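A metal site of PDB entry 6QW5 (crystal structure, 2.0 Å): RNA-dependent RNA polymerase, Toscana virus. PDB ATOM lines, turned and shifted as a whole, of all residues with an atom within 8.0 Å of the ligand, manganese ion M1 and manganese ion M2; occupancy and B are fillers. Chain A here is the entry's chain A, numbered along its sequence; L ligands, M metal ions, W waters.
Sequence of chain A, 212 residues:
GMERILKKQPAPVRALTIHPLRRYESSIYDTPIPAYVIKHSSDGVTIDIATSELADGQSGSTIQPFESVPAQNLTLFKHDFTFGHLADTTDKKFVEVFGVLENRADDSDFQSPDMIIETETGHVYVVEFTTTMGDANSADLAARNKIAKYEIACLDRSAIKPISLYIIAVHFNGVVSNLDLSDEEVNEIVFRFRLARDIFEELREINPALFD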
ATOM      1  N   THR A  75      -7.825 -21.348   9.641  1.00  0.00           N
ATOM      2  CA  THR A  75      -7.334 -19.978   9.811  1.00  0.00           C
ATOM      3  C   THR A  75      -7.231 -19.578  11.277  1.00  0.00           C
ATOM      4  O   THR A  75      -6.489 -18.646  11.614  1.00  0.00           O
ATOM      5  CB  THR A  75      -8.251 -18.989   9.083  1.00  0.00           C
ATOM      6  OG1 THR A  75      -9.563 -19.087   9.636  1.00  0.00           O
ATOM      7  CG2 THR A  75      -8.323 -19.303   7.605  1.00  0.00           C
ATOM      8  N   LEU A  76      -7.964 -20.254  12.164  1.00  0.00           N
ATOM      9  CA  LEU A  76      -7.886 -19.955  13.587  1.00  0.00           C
ATOM     10  C   LEU A  76      -7.105 -21.015  14.354  1.00  0.00           C
ATOM     11  O   LEU A  76      -7.256 -21.133  15.567  1.00  0.00           O
ATOM     12  CB  LEU A  76      -9.297 -19.792  14.162  1.00  0.00           C
ATOM     13  CG  LEU A  76      -9.986 -18.496  13.736  1.00  0.00           C
ATOM     14  CD1 LEU A  76     -11.283 -18.303  14.527  1.00  0.00           C
ATOM     15  CD2 LEU A  76      -9.063 -17.293  13.901  1.00  0.00           C
ATOM     16  N   HIS A  79      -4.933 -19.774  17.424  1.00  0.00           N
ATOM     17  CA  HIS A  79      -5.853 -19.427  18.504  1.00  0.00           C
ATOM     18  C   HIS A  79      -6.501 -20.690  19.074  1.00  0.00           C
ATOM     19  O   HIS A  79      -6.443 -20.927  20.288  1.00  0.00           O
ATOM     20  CB  HIS A  79      -6.879 -18.435  17.945  1.00  0.00           C
ATOM     21  CG  HIS A  79      -7.988 -18.058  18.875  1.00  0.00           C
ATOM     22  ND1 HIS A  79      -9.101 -18.845  19.055  1.00  0.00           N
ATOM     23  CD2 HIS A  79      -8.188 -16.937  19.604  1.00  0.00           C
ATOM     24  CE1 HIS A  79      -9.939 -18.246  19.886  1.00  0.00           C
ATOM     25  NE2 HIS A  79      -9.409 -17.084  20.230  1.00  0.00           N
ATOM     26  N   ASP A  80      -7.042 -21.547  18.219  1.00  0.00           N
ATOM     27  CA  ASP A  80      -7.826 -22.672  18.726  1.00  0.00           C
ATOM     28  C   ASP A  80      -6.972 -23.809  19.277  1.00  0.00           C
ATOM     29  O   ASP A  80      -7.333 -24.412  20.293  1.00  0.00           O
ATOM     30  CB  ASP A  80      -8.759 -23.170  17.634  1.00  0.00           C
ATOM     31  CG  ASP A  80      -9.878 -22.174  17.342  1.00  0.00           C
ATOM     32  OD1 ASP A  80     -10.456 -21.604  18.313  1.00  0.00           O
ATOM     33  OD2 ASP A  80     -10.151 -21.957  16.151  1.00  0.00           O
ATOM     34  N   PHE A  83      -5.846 -22.926  23.019  1.00  0.00           N
ATOM     35  CA  PHE A  83      -6.851 -23.056  24.075  1.00  0.00           C
ATOM     36  C   PHE A  83      -7.754 -24.275  23.874  1.00  0.00           C
ATOM     37  O   PHE A  83      -8.857 -24.314  24.421  1.00  0.00           O
ATOM     38  CB  PHE A  83      -7.685 -21.764  24.159  1.00  0.00           C
ATOM     39  CG  PHE A  83      -6.852 -20.529  24.380  1.00  0.00           C
ATOM     40  CD1 PHE A  83      -6.433 -20.179  25.652  1.00  0.00           C
ATOM     41  CD2 PHE A  83      -6.449 -19.746  23.307  1.00  0.00           C
ATOM     42  CE1 PHE A  83      -5.651 -19.051  25.864  1.00  0.00           C
ATOM     43  CE2 PHE A  83      -5.680 -18.600  23.509  1.00  0.00           C
ATOM     44  CZ  PHE A  83      -5.274 -18.251  24.786  1.00  0.00           C
ATOM     45  N   THR A  89     -14.740 -26.249  21.243  1.00  0.00           N
ATOM     46  CA  THR A  89     -14.859 -25.302  20.148  1.00  0.00           C
ATOM     47  C   THR A  89     -14.948 -23.919  20.788  1.00  0.00           C
ATOM     48  O   THR A  89     -15.060 -23.788  22.005  1.00  0.00           O
ATOM     49  CB  THR A  89     -16.108 -25.589  19.312  1.00  0.00           C
ATOM     50  OG1 THR A  89     -16.392 -24.451  18.469  1.00  0.00           O
ATOM     51  CG2 THR A  89     -17.296 -25.853  20.221  1.00  0.00           C
ATOM     52  N   THR A  90     -14.930 -22.878  19.957  1.00  0.00           N
ATOM     53  CA  THR A  90     -15.165 -21.533  20.459  1.00  0.00           C
ATOM     54  C   THR A  90     -16.284 -20.870  19.661  1.00  0.00           C
ATOM     55  O   THR A  90     -16.866 -21.465  18.736  1.00  0.00           O
ATOM     56  CB  THR A  90     -13.885 -20.679  20.444  1.00  0.00           C
ATOM     57  OG1 THR A  90     -13.300 -20.687  19.136  1.00  0.00           O
ATOM     58  CG2 THR A  90     -12.871 -21.182  21.460  1.00  0.00           C
ATOM     59  N   ASP A  91     -16.600 -19.634  20.061  1.00  0.00           N
ATOM     60  CA  ASP A  91     -17.616 -18.770  19.464  1.00  0.00           C
ATOM     61  C   ASP A  91     -19.045 -19.267  19.701  1.00  0.00           C
ATOM     62  O   ASP A  91     -19.501 -20.223  19.067  1.00  0.00           O
ATOM     63  CB  ASP A  91     -17.330 -18.587  17.981  1.00  0.00           C
ATOM     64  CG  ASP A  91     -16.000 -17.886  17.723  1.00  0.00           C
ATOM     65  OD1 ASP A  91     -15.342 -17.435  18.688  1.00  0.00           O
ATOM     66  OD2 ASP A  91     -15.588 -17.783  16.544  1.00  0.00           O
ATOM     67  N   LYS A  92     -19.764 -18.601  20.621  1.00  0.00           N
ATOM     68  CA  LYS A  92     -21.197 -18.770  20.830  1.00  0.00           C
ATOM     69  C   LYS A  92     -21.843 -17.394  20.784  1.00  0.00           C
ATOM     70  O   LYS A  92     -21.356 -16.462  21.435  1.00  0.00           O
ATOM     71  CB  LYS A  92     -21.488 -19.436  22.190  1.00  0.00           C
ATOM     72  CG  LYS A  92     -22.923 -19.893  22.358  1.00  0.00           C
ATOM     73  CD  LYS A  92     -23.059 -20.987  23.398  1.00  0.00           C
ATOM     74  CE  LYS A  92     -24.288 -21.828  23.121  1.00  0.00           C
ATOM     75  NZ  LYS A  92     -24.415 -22.998  24.050  1.00  0.00           N
ATOM     76  N   SER A 112     -20.030 -13.025  19.163  1.00  0.00           N
ATOM     77  CA  SER A 112     -19.815 -14.392  19.608  1.00  0.00           C
ATOM     78  C   SER A 112     -18.448 -14.508  20.268  1.00  0.00           C
ATOM     79  O   SER A 112     -17.449 -14.808  19.621  1.00  0.00           O
ATOM     80  CB  SER A 112     -19.932 -15.391  18.444  1.00  0.00           C
ATOM     81  OG  SER A 112     -19.210 -14.922  17.314  1.00  0.00           O
ATOM     82  N   PRO A 113     -18.391 -14.272  21.583  1.00  0.00           N
ATOM     83  CA  PRO A 113     -17.135 -14.532  22.306  1.00  0.00           C
ATOM     84  C   PRO A 113     -16.833 -16.023  22.291  1.00  0.00           C
ATOM     85  O   PRO A 113     -17.654 -16.846  21.894  1.00  0.00           O
ATOM     86  CB  PRO A 113     -17.396 -13.996  23.721  1.00  0.00           C
ATOM     87  CG  PRO A 113     -18.888 -13.797  23.818  1.00  0.00           C
ATOM     88  CD  PRO A 113     -19.454 -13.729  22.437  1.00  0.00           C
ATOM     89  N   ASP A 114     -15.603 -16.368  22.703  1.00  0.00           N
ATOM     90  CA  ASP A 114     -15.148 -17.749  22.579  1.00  0.00           C
ATOM     91  C   ASP A 114     -15.957 -18.701  23.453  1.00  0.00           C
ATOM     92  O   ASP A 114     -16.120 -19.863  23.083  1.00  0.00           O
ATOM     93  CB  ASP A 114     -13.655 -17.846  22.928  1.00  0.00           C
ATOM     94  CG  ASP A 114     -12.773 -17.273  21.840  1.00  0.00           C
ATOM     95  OD1 ASP A 114     -13.107 -17.392  20.637  1.00  0.00           O
ATOM     96  OD2 ASP A 114     -11.745 -16.671  22.195  1.00  0.00           O
ATOM     97  N   MET A 115     -16.434 -18.257  24.612  1.00  0.00           N
ATOM     98  CA  MET A 115     -17.307 -19.101  25.447  1.00  0.00           C
ATOM     99  C   MET A 115     -18.401 -18.264  26.114  1.00  0.00           C
ATOM    100  O   MET A 115     -18.161 -17.141  26.544  1.00  0.00           O
ATOM    101  CB  MET A 115     -16.525 -19.847  26.532  1.00  0.00           C
ATOM    102  CG  MET A 115     -15.260 -20.588  26.098  1.00  0.00           C
ATOM    103  SD  MET A 115     -14.469 -21.544  27.630  1.00  0.00           S
ATOM    104  CE  MET A 115     -15.527 -23.209  27.522  1.00  0.00           C
ATOM    105  N   VAL A 127     -16.204 -15.772  28.206  1.00  0.00           N
ATOM    106  CA  VAL A 127     -14.747 -16.003  28.149  1.00  0.00           C
ATOM    107  C   VAL A 127     -14.232 -15.687  26.749  1.00  0.00           C
ATOM    108  O   VAL A 127     -14.772 -16.190  25.757  1.00  0.00           O
ATOM    109  CB  VAL A 127     -14.363 -17.440  28.535  1.00  0.00           C
ATOM    110  CG1 VAL A 127     -12.834 -17.565  28.687  1.00  0.00           C
ATOM    111  CG2 VAL A 127     -15.078 -17.906  29.820  1.00  0.00           C
ATOM    112  N   GLU A 128     -13.194 -14.861  26.650  1.00  0.00           N
ATOM    113  CA  GLU A 128     -12.568 -14.584  25.365  1.00  0.00           C
ATOM    114  C   GLU A 128     -11.083 -14.910  25.449  1.00  0.00           C
ATOM    115  O   GLU A 128     -10.428 -14.532  26.423  1.00  0.00           O
ATOM    116  CB  GLU A 128     -12.772 -13.146  24.915  1.00  0.00           C
ATOM    117  CG  GLU A 128     -12.110 -12.807  23.557  1.00  0.00           C
ATOM    118  CD  GLU A 128     -12.684 -13.575  22.367  1.00  0.00           C
ATOM    119  OE1 GLU A 128     -13.832 -14.067  22.459  1.00  0.00           O
ATOM    120  OE2 GLU A 128     -11.993 -13.691  21.336  1.00  0.00           O
ATOM    121  N   PHE A 129     -10.598 -15.635  24.458  1.00  0.00           N
ATOM    122  CA  PHE A 129      -9.186 -15.965  24.297  1.00  0.00           C
ATOM    123  C   PHE A 129      -8.565 -15.107  23.207  1.00  0.00           C
ATOM    124  O   PHE A 129      -9.198 -14.782  22.192  1.00  0.00           O
ATOM    125  CB  PHE A 129      -8.988 -17.441  23.907  1.00  0.00           C
ATOM    126  CG  PHE A 129      -9.751 -18.425  24.751  1.00  0.00           C
ATOM    127  CD1 PHE A 129      -9.599 -18.437  26.124  1.00  0.00           C
ATOM    128  CD2 PHE A 129     -10.594 -19.363  24.154  1.00  0.00           C
ATOM    129  CE1 PHE A 129     -10.285 -19.357  26.906  1.00  0.00           C
ATOM    130  CE2 PHE A 129     -11.289 -20.280  24.933  1.00  0.00           C
ATOM    131  CZ  PHE A 129     -11.133 -20.279  26.303  1.00  0.00           C
ATOM    132  N   THR A 130      -7.285 -14.808  23.374  1.00  0.00           N
ATOM    133  CA  THR A 130      -6.570 -14.090  22.336  1.00  0.00           C
ATOM    134  C   THR A 130      -5.086 -14.408  22.486  1.00  0.00           C
ATOM    135  O   THR A 130      -4.646 -14.930  23.505  1.00  0.00           O
ATOM    136  CB  THR A 130      -6.864 -12.577  22.431  1.00  0.00           C
ATOM    137  OG1 THR A 130      -6.358 -11.901  21.269  1.00  0.00           O
ATOM    138  CG2 THR A 130      -6.264 -11.983  23.680  1.00  0.00           C
ATOM    139  N   THR A 131      -4.340 -14.150  21.421  1.00  0.00           N
ATOM    140  CA  THR A 131      -2.903 -14.413  21.361  1.00  0.00           C
ATOM    141  C   THR A 131      -2.210 -13.172  20.804  1.00  0.00           C
ATOM    142  O   THR A 131      -2.839 -12.326  20.170  1.00  0.00           O
ATOM    143  CB  THR A 131      -2.570 -15.617  20.459  1.00  0.00           C
ATOM    144  OG1 THR A 131      -2.615 -15.214  19.076  1.00  0.00           O
ATOM    145  CG2 THR A 131      -3.564 -16.741  20.649  1.00  0.00           C
ATOM    146  N   ALA A 142      -3.846  -6.635  24.184  1.00  0.00           N
ATOM    147  CA  ALA A 142      -4.814  -7.488  23.514  1.00  0.00           C
ATOM    148  C   ALA A 142      -5.971  -7.873  24.450  1.00  0.00           C
ATOM    149  O   ALA A 142      -7.128  -7.907  24.026  1.00  0.00           O
ATOM    150  CB  ALA A 142      -4.124  -8.746  22.966  1.00  0.00           C
ATOM    151  N   LYS A 146      -9.998  -7.009  23.958  1.00  0.00           N
ATOM    152  CA  LYS A 146     -11.132  -7.935  24.001  1.00  0.00           C
ATOM    153  C   LYS A 146     -12.184  -7.483  25.015  1.00  0.00           C
ATOM    154  O   LYS A 146     -13.389  -7.648  24.785  1.00  0.00           O
ATOM    155  CB  LYS A 146     -10.659  -9.354  24.345  1.00  0.00           C
ATOM    156  CG  LYS A 146      -9.807 -10.008  23.265  1.00  0.00           C
ATOM    157  CD  LYS A 146     -10.472  -9.883  21.899  1.00  0.00           C
ATOM    158  CE  LYS A 146      -9.759 -10.760  20.863  1.00  0.00           C
ATOM    159  NZ  LYS A 146     -10.441 -10.722  19.529  1.00  0.00           N
ATOM    160  N   LYS A 149     -14.106  -4.839  23.314  1.00  0.00           N
ATOM    161  CA  LYS A 149     -14.950  -5.372  22.253  1.00  0.00           C
ATOM    162  C   LYS A 149     -16.267  -5.939  22.778  1.00  0.00           C
ATOM    163  O   LYS A 149     -17.295  -5.843  22.092  1.00  0.00           O
ATOM    164  CB  LYS A 149     -14.171  -6.450  21.498  1.00  0.00           C
ATOM    165  CG  LYS A 149     -14.962  -7.213  20.469  1.00  0.00           C
ATOM    166  CD  LYS A 149     -14.080  -8.281  19.827  1.00  0.00           C
ATOM    167  CE  LYS A 149     -14.747  -8.942  18.644  1.00  0.00           C
ATOM    168  NZ  LYS A 149     -14.869  -7.999  17.495  1.00  0.00           N
ATOM    169  N   TYR A 150     -16.279  -6.518  23.973  1.00  0.00           N
ATOM    170  CA  TYR A 150     -17.469  -7.206  24.453  1.00  0.00           C
ATOM    171  C   TYR A 150     -18.136  -6.547  25.661  1.00  0.00           C
ATOM    172  O   TYR A 150     -19.211  -6.997  26.054  1.00  0.00           O
ATOM    173  CB  TYR A 150     -17.132  -8.673  24.796  1.00  0.00           C
ATOM    174  CG  TYR A 150     -16.783  -9.506  23.586  1.00  0.00           C
ATOM    175  CD1 TYR A 150     -17.728  -9.800  22.623  1.00  0.00           C
ATOM    176  CD2 TYR A 150     -15.491  -9.983  23.395  1.00  0.00           C
ATOM    177  CE1 TYR A 150     -17.412 -10.561  21.495  1.00  0.00           C
ATOM    178  CE2 TYR A 150     -15.152 -10.737  22.271  1.00  0.00           C
ATOM    179  CZ  TYR A 150     -16.119 -11.033  21.333  1.00  0.00           C
ATOM    180  OH  TYR A 150     -15.802 -11.777  20.215  1.00  0.00           O
ATOM    181  N   ILE A 168      -8.192 -14.474  28.608  1.00  0.00           N
ATOM    182  CA  ILE A 168      -6.852 -15.057  28.613  1.00  0.00           C
ATOM    183  C   ILE A 168      -6.140 -14.586  27.341  1.00  0.00           C
ATOM    184  O   ILE A 168      -6.578 -14.908  26.224  1.00  0.00           O
ATOM    185  CB  ILE A 168      -6.867 -16.597  28.663  1.00  0.00           C
ATOM    186  CG1 ILE A 168      -7.786 -17.137  29.760  1.00  0.00           C
ATOM    187  CG2 ILE A 168      -5.438 -17.132  28.818  1.00  0.00           C
ATOM    188  CD1 ILE A 168      -7.806 -18.690  29.813  1.00  0.00           C
HETATM  189  O1  LIG L   1     -11.782 -15.495  18.977  1.00  0.00           O
HETATM  190  C1  LIG L   1     -11.207 -14.700  18.042  1.00  0.00           C
HETATM  191  C2  LIG L   1     -10.093 -13.957  18.343  1.00  0.00           C
HETATM  192  O2  LIG L   1      -9.496 -13.996  19.466  1.00  0.00           O
HETATM  193  O3  LIG L   1      -9.618 -13.176  17.484  1.00  0.00           O
HETATM  194  C3  LIG L   1     -11.725 -14.604  16.790  1.00  0.00           C
HETATM  195  C4  LIG L   1     -12.932 -15.297  16.252  1.00  0.00           C
HETATM  196  C5  LIG L   1     -13.257 -15.160  14.763  1.00  0.00           C
HETATM  197  C6  LIG L   1     -12.472 -14.306  13.962  1.00  0.00           C
HETATM  198  C7  LIG L   1     -12.737 -14.140  12.597  1.00  0.00           C
HETATM  199  C8  LIG L   1     -13.798 -14.832  12.000  1.00  0.00           C
HETATM  200  C9  LIG L   1     -14.583 -15.686  12.801  1.00  0.00           C
HETATM  201  C10 LIG L   1     -14.317 -15.843  14.171  1.00  0.00           C
HETATM  202  O4  LIG L   1     -13.797 -15.851  16.943  1.00  0.00           O
HETATM  203 MN    MN M   1     -10.650 -15.318  20.747  1.00  0.00          MN
HETATM  204 MN    MN M   2     -13.497 -16.596  18.811  1.00  0.00          MN
HETATM  205  O   HOH W   1     -12.708 -18.320  18.056  1.00  0.00           O
HETATM  206  O   HOH W   2     -16.637 -15.331  16.626  1.00  0.00           O
HETATM  207  O   HOH W   3      -7.166 -12.946  18.960  1.00  0.00           O
HETATM  208  O   HOH W   4      -8.079 -11.002  17.511  1.00  0.00           O
HETATM  209  O   HOH W   5     -14.597 -14.904  19.681  1.00  0.00           O
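Of the 23 residues printed, 2 come within 4 Å of manganese ion M2.
Along chain A the residues within 4 Å of manganese ion M2 span positions 91 to 114.
The nearest printed residue that does not touch manganese ion M2 is His 79 (4.1 Å).
The backbone NH (N) of Asp 114 lies within hydrogen-bond range of the backbone carbonyl oxygen (O) of Val 127, at 3.2 Å.
N of Asp 91 sits close to O of Pro 113, at 3.5 Å.
NZ of Lys 146 lies close to OE2 of Glu 128 (3.8 Å).
The backbone carbonyl oxygen (O) of Glu 128 is in hydrogen-bond range of the backbone NH (N) of Ile 168, at 3.1 Å.
A ring nitrogen (ND1) of His 79 lies within hydrogen-bond range of the side-chain carboxylate of Asp 80.
NZ of Lys 146 is in salt-bridge range of O3 of the ligand (3.3 Å).
An oxygen (O1) of the ligand is bound to manganese ion M1, at 2.1 Å.
Manganese ion M1 is bound by O of Phe 129 (2.1 Å).
O2 of the ligand binds manganese ion M1 (2.2 Å).
The side-chain carboxylate (OE2) of Glu 128 binds manganese ion M1, at 2.2 Å.
Manganese ion M1 is bound by NE2 of His 79.
OD2 of Asp 114 binds manganese ion M1, 2.3 Å away.
Manganese ion M1 has six donor atoms within binding distance.
Water W5 lies within hydrogen-bond range of O of Ser 112 (2.9 Å), OE1 of Glu 128 (3.0 Å) and OH of Tyr 150 (3.4 Å).
Water W1 bridges OG1 of Thr 90 (2.7 Å) and OD2 of Asp 91 (3.3 Å).
Water W3 lies within hydrogen-bond range of the side-chain hydroxyl of Thr 130 (2.7 Å) and an oxygen (O3) of the ligand (2.9 Å).
Water W4 lies within hydrogen-bond range of O3 of the ligand and NZ of Lys 146.
Water W2 lies within hydrogen-bond range of the side-chain carboxylate of Asp 91 (2.7 Å) and the side-chain hydroxyl of Ser 112 (2.7 Å).
Residues that only touch the ligand: Leu 76.
Hydrophobic or aromatic side chains within 4 Å of the ligand: Leu 76 and His 79.
Within 4 Å of the ligand: Leu 76, His 79, Asp 91, Asp 114, Glu 128, Phe 129 and Lys 146.
Within 4 Å of manganese ion M1: His 79, Asp 114, Glu 128 and Phe 129.
Along chain A the residues within 4 Å of manganese ion M1 span positions 79 to 129.
Manganese ion M2 is bound by OD1 of Asp 114 (2.0 Å), OD1 of Asp 91 (2.0 Å), O4 of the ligand (2.0 Å), water W1 (2.0 Å), O1 of the ligand (2.0 Å) and water W5 (2.2 Å).
Manganese ion M2 has six donor atoms within binding distance.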
